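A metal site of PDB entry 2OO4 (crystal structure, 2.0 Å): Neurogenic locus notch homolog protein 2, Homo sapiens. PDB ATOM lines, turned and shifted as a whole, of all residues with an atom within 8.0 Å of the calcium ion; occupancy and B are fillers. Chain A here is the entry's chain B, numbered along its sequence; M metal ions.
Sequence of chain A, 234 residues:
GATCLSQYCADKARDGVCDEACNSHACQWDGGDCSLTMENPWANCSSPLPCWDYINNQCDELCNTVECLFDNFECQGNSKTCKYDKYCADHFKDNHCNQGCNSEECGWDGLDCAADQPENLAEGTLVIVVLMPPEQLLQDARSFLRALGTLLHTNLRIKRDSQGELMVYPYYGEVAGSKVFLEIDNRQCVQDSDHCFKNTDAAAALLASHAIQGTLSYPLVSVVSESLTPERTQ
Residues that only touch the calcium ion: Lys 12 (3.8 Å) and Ala 13 (3.9 Å).
Within 4 Å of the calcium ion: Lys 12, Ala 13, Asp 15, Val 17, Asp 19, Asp 30 and Asp 33.
The nearest printed residue that does not touch the calcium ion is Cys 18 (4.6 Å).
The calcium ion is bound by OD2 of Asp 30 (2.3 Å), OD2 of Asp 19 (2.4 Å), OD2 of Asp 33 (2.4 Å), OD1 of Asp 15 (2.5 Å) and O of Val 17 (2.5 Å).
The calcium ion has five donor atoms within binding distance.
The side-chain sulfur (SG) of Cys 22 forms a disulfide with the side-chain sulfur (SG) of Cys 9, 2.1 Å away.
The side-chain carboxylate (OD1) of Asp 30 sits close to the backbone carbonyl oxygen (O) of Lys 12 (2.7 Å).
The backbone carbonyl oxygen (O) of Cys 22 sits at hydrogen-bond distance from the backbone NH (N) of Asp 30, 3.0 Å away.
SG of Cys 18 forms a disulfide with SG of Cys 34.
The backbone NH (N) of Ala 13 sits close to the side-chain carboxylate (OD1) of Asp 15.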
ATOM      1  N   TYR A   8     -21.207  -3.649   5.186  1.00  0.00           N
ATOM      2  CA  TYR A   8     -21.410  -3.915   3.759  1.00  0.00           C
ATOM      3  C   TYR A   8     -22.797  -4.481   3.456  1.00  0.00           C
ATOM      4  O   TYR A   8     -23.393  -4.159   2.425  1.00  0.00           O
ATOM      5  CB  TYR A   8     -20.331  -4.839   3.226  1.00  0.00           C
ATOM      6  N   CYS A   9     -23.314  -5.326   4.351  1.00  0.00           N
ATOM      7  CA  CYS A   9     -24.604  -5.990   4.143  1.00  0.00           C
ATOM      8  C   CYS A   9     -25.817  -5.147   4.492  1.00  0.00           C
ATOM      9  O   CYS A   9     -26.944  -5.478   4.091  1.00  0.00           O
ATOM     10  CB  CYS A   9     -24.640  -7.329   4.881  1.00  0.00           C
ATOM     11  SG  CYS A   9     -23.660  -8.625   4.090  1.00  0.00           S
ATOM     12  N   ASP A  11     -26.018  -1.815   3.632  1.00  0.00           N
ATOM     13  CA  ASP A  11     -26.193  -0.983   2.437  1.00  0.00           C
ATOM     14  C   ASP A  11     -26.720  -1.773   1.249  1.00  0.00           C
ATOM     15  O   ASP A  11     -27.367  -1.220   0.356  1.00  0.00           O
ATOM     16  CB  ASP A  11     -24.862  -0.308   2.069  1.00  0.00           C
ATOM     17  CG  ASP A  11     -25.032   0.837   1.084  1.00  0.00           C
ATOM     18  OD1 ASP A  11     -25.591   1.892   1.481  1.00  0.00           O
ATOM     19  OD2 ASP A  11     -24.608   0.690  -0.082  1.00  0.00           O
ATOM     20  N   LYS A  12     -26.440  -3.088   1.249  1.00  0.00           N
ATOM     21  CA  LYS A  12     -26.922  -3.990   0.207  1.00  0.00           C
ATOM     22  C   LYS A  12     -28.163  -4.765   0.663  1.00  0.00           C
ATOM     23  O   LYS A  12     -28.074  -5.660   1.516  1.00  0.00           O
ATOM     24  CB  LYS A  12     -25.809  -4.954  -0.216  1.00  0.00           C
ATOM     25  N   ALA A  13     -29.316  -4.411   0.094  1.00  0.00           N
ATOM     26  CA  ALA A  13     -30.592  -5.037   0.448  1.00  0.00           C
ATOM     27  C   ALA A  13     -31.677  -4.842  -0.613  1.00  0.00           C
ATOM     28  O   ALA A  13     -32.460  -5.759  -0.889  1.00  0.00           O
ATOM     29  CB  ALA A  13     -31.086  -4.551   1.814  1.00  0.00           C
ATOM     30  N   ARG A  14     -31.731  -3.639  -1.195  1.00  0.00           N
ATOM     31  CA  ARG A  14     -32.754  -3.291  -2.191  1.00  0.00           C
ATOM     32  C   ARG A  14     -32.243  -3.452  -3.617  1.00  0.00           C
ATOM     33  O   ARG A  14     -32.991  -3.893  -4.503  1.00  0.00           O
ATOM     34  CB  ARG A  14     -33.260  -1.856  -1.958  1.00  0.00           C
ATOM     35  CG  ARG A  14     -34.142  -1.304  -3.075  1.00  0.00           C
ATOM     36  CD  ARG A  14     -34.275   0.205  -2.994  1.00  0.00           C
ATOM     37  NE  ARG A  14     -35.549   0.611  -2.410  1.00  0.00           N
ATOM     38  CZ  ARG A  14     -36.634   0.943  -3.120  1.00  0.00           C
ATOM     39  NH1 ARG A  14     -36.612   0.909  -4.443  1.00  0.00           N
ATOM     40  NH2 ARG A  14     -37.744   1.302  -2.487  1.00  0.00           N
ATOM     41  N   ASP A  15     -30.972  -3.111  -3.839  1.00  0.00           N
ATOM     42  CA  ASP A  15     -30.367  -3.100  -5.180  1.00  0.00           C
ATOM     43  C   ASP A  15     -30.533  -4.408  -5.944  1.00  0.00           C
ATOM     44  O   ASP A  15     -30.511  -5.500  -5.362  1.00  0.00           O
ATOM     45  CB  ASP A  15     -28.876  -2.722  -5.088  1.00  0.00           C
ATOM     46  CG  ASP A  15     -28.074  -3.648  -4.189  1.00  0.00           C
ATOM     47  OD1 ASP A  15     -28.671  -4.311  -3.301  1.00  0.00           O
ATOM     48  OD2 ASP A  15     -26.842  -3.739  -4.363  1.00  0.00           O
ATOM     49  N   GLY A  16     -30.705  -4.298  -7.269  1.00  0.00           N
ATOM     50  CA  GLY A  16     -30.918  -5.462  -8.134  1.00  0.00           C
ATOM     51  C   GLY A  16     -29.666  -6.285  -8.376  1.00  0.00           C
ATOM     52  O   GLY A  16     -29.371  -6.662  -9.509  1.00  0.00           O
ATOM     53  N   VAL A  17     -28.931  -6.562  -7.301  1.00  0.00           N
ATOM     54  CA  VAL A  17     -27.705  -7.356  -7.327  1.00  0.00           C
ATOM     55  C   VAL A  17     -27.679  -8.307  -6.130  1.00  0.00           C
ATOM     56  O   VAL A  17     -27.916  -7.871  -5.002  1.00  0.00           O
ATOM     57  CB  VAL A  17     -26.433  -6.456  -7.308  1.00  0.00           C
ATOM     58  CG1 VAL A  17     -25.163  -7.300  -7.169  1.00  0.00           C
ATOM     59  CG2 VAL A  17     -26.348  -5.591  -8.556  1.00  0.00           C
ATOM     60  N   CYS A  18     -27.409  -9.577  -6.383  1.00  0.00           N
ATOM     61  CA  CYS A  18     -27.178 -10.543  -5.306  1.00  0.00           C
ATOM     62  C   CYS A  18     -25.729 -10.497  -4.851  1.00  0.00           C
ATOM     63  O   CYS A  18     -24.845 -11.068  -5.497  1.00  0.00           O
ATOM     64  CB  CYS A  18     -27.568 -11.962  -5.725  1.00  0.00           C
ATOM     65  SG  CYS A  18     -27.048 -13.251  -4.545  1.00  0.00           S
ATOM     66  N   ASP A  19     -25.492  -9.789  -3.756  1.00  0.00           N
ATOM     67  CA  ASP A  19     -24.162  -9.724  -3.144  1.00  0.00           C
ATOM     68  C   ASP A  19     -23.990 -10.967  -2.283  1.00  0.00           C
ATOM     69  O   ASP A  19     -24.642 -11.104  -1.239  1.00  0.00           O
ATOM     70  CB  ASP A  19     -24.002  -8.447  -2.320  1.00  0.00           C
ATOM     71  CG  ASP A  19     -24.387  -7.199  -3.114  1.00  0.00           C
ATOM     72  OD1 ASP A  19     -23.481  -6.467  -3.550  1.00  0.00           O
ATOM     73  OD2 ASP A  19     -25.605  -6.959  -3.292  1.00  0.00           O
ATOM     74  N   GLU A  20     -23.145 -11.875  -2.743  1.00  0.00           N
ATOM     75  CA  GLU A  20     -23.036 -13.221  -2.164  1.00  0.00           C
ATOM     76  C   GLU A  20     -22.445 -13.228  -0.751  1.00  0.00           C
ATOM     77  O   GLU A  20     -22.601 -14.203  -0.011  1.00  0.00           O
ATOM     78  CB  GLU A  20     -22.250 -14.154  -3.102  1.00  0.00           C
ATOM     79  CG  GLU A  20     -22.279 -15.647  -2.720  1.00  0.00           C
ATOM     80  CD  GLU A  20     -23.667 -16.276  -2.801  1.00  0.00           C
ATOM     81  OE1 GLU A  20     -24.461 -15.918  -3.696  1.00  0.00           O
ATOM     82  OE2 GLU A  20     -23.955 -17.158  -1.954  1.00  0.00           O
ATOM     83  N   CYS A  22     -23.635 -11.541   1.448  1.00  0.00           N
ATOM     84  CA  CYS A  22     -24.829 -11.311   2.259  1.00  0.00           C
ATOM     85  C   CYS A  22     -25.898 -12.391   2.065  1.00  0.00           C
ATOM     86  O   CYS A  22     -26.993 -12.309   2.631  1.00  0.00           O
ATOM     87  CB  CYS A  22     -25.411  -9.926   1.960  1.00  0.00           C
ATOM     88  SG  CYS A  22     -24.238  -8.559   2.123  1.00  0.00           S
ATOM     89  N   TRP A  29     -31.100 -13.362   3.086  1.00  0.00           N
ATOM     90  CA  TRP A  29     -30.498 -13.571   1.766  1.00  0.00           C
ATOM     91  C   TRP A  29     -30.405 -12.288   0.955  1.00  0.00           C
ATOM     92  O   TRP A  29     -31.007 -12.157  -0.123  1.00  0.00           O
ATOM     93  CB  TRP A  29     -31.222 -14.696   1.004  1.00  0.00           C
ATOM     94  CG  TRP A  29     -31.182 -15.996   1.752  1.00  0.00           C
ATOM     95  CD1 TRP A  29     -30.113 -16.848   1.865  1.00  0.00           C
ATOM     96  CD2 TRP A  29     -32.238 -16.570   2.526  1.00  0.00           C
ATOM     97  NE1 TRP A  29     -30.450 -17.932   2.643  1.00  0.00           N
ATOM     98  CE2 TRP A  29     -31.747 -17.790   3.058  1.00  0.00           C
ATOM     99  CE3 TRP A  29     -33.550 -16.186   2.811  1.00  0.00           C
ATOM    100  CZ2 TRP A  29     -32.526 -18.619   3.870  1.00  0.00           C
ATOM    101  CZ3 TRP A  29     -34.329 -17.015   3.623  1.00  0.00           C
ATOM    102  CH2 TRP A  29     -33.809 -18.217   4.132  1.00  0.00           C
ATOM    103  N   ASP A  30     -29.633 -11.349   1.493  1.00  0.00           N
ATOM    104  CA  ASP A  30     -29.392 -10.024   0.907  1.00  0.00           C
ATOM    105  C   ASP A  30     -30.685  -9.203   0.738  1.00  0.00           C
ATOM    106  O   ASP A  30     -30.814  -8.411  -0.203  1.00  0.00           O
ATOM    107  CB  ASP A  30     -28.615 -10.139  -0.409  1.00  0.00           C
ATOM    108  CG  ASP A  30     -27.956  -8.836  -0.815  1.00  0.00           C
ATOM    109  OD1 ASP A  30     -27.823  -7.934   0.031  1.00  0.00           O
ATOM    110  OD2 ASP A  30     -27.550  -8.709  -1.987  1.00  0.00           O
ATOM    111  N   GLY A  31     -31.612  -9.387   1.666  1.00  0.00           N
ATOM    112  CA  GLY A  31     -32.902  -8.705   1.636  1.00  0.00           C
ATOM    113  C   GLY A  31     -33.757  -9.080   0.438  1.00  0.00           C
ATOM    114  O   GLY A  31     -34.448  -8.238  -0.116  1.00  0.00           O
ATOM    115  N   GLY A  32     -33.690 -10.353   0.052  1.00  0.00           N
ATOM    116  CA  GLY A  32     -34.480 -10.881  -1.065  1.00  0.00           C
ATOM    117  C   GLY A  32     -33.788 -10.912  -2.407  1.00  0.00           C
ATOM    118  O   GLY A  32     -34.235 -11.621  -3.327  1.00  0.00           O
ATOM    119  N   ASP A  33     -32.689 -10.175  -2.539  1.00  0.00           N
ATOM    120  CA  ASP A  33     -31.968 -10.065  -3.821  1.00  0.00           C
ATOM    121  C   ASP A  33     -31.468 -11.404  -4.369  1.00  0.00           C
ATOM    122  O   ASP A  33     -31.366 -11.581  -5.581  1.00  0.00           O
ATOM    123  CB  ASP A  33     -30.785  -9.099  -3.692  1.00  0.00           C
ATOM    124  CG  ASP A  33     -31.210  -7.691  -3.281  1.00  0.00           C
ATOM    125  OD1 ASP A  33     -32.370  -7.311  -3.514  1.00  0.00           O
ATOM    126  OD2 ASP A  33     -30.356  -6.971  -2.714  1.00  0.00           O
ATOM    127  N   CYS A  34     -31.139 -12.325  -3.468  1.00  0.00           N
ATOM    128  CA  CYS A  34     -30.595 -13.641  -3.836  1.00  0.00           C
ATOM    129  C   CYS A  34     -31.652 -14.739  -3.787  1.00  0.00           C
ATOM    130  O   CYS A  34     -31.378 -15.892  -4.134  1.00  0.00           O
ATOM    131  CB  CYS A  34     -29.452 -14.011  -2.903  1.00  0.00           C
ATOM    132  SG  CYS A  34     -28.086 -12.823  -2.855  1.00  0.00           S
HETATM  133 CA    CA M   1     -27.948  -6.611  -2.844  1.00  0.00          CA
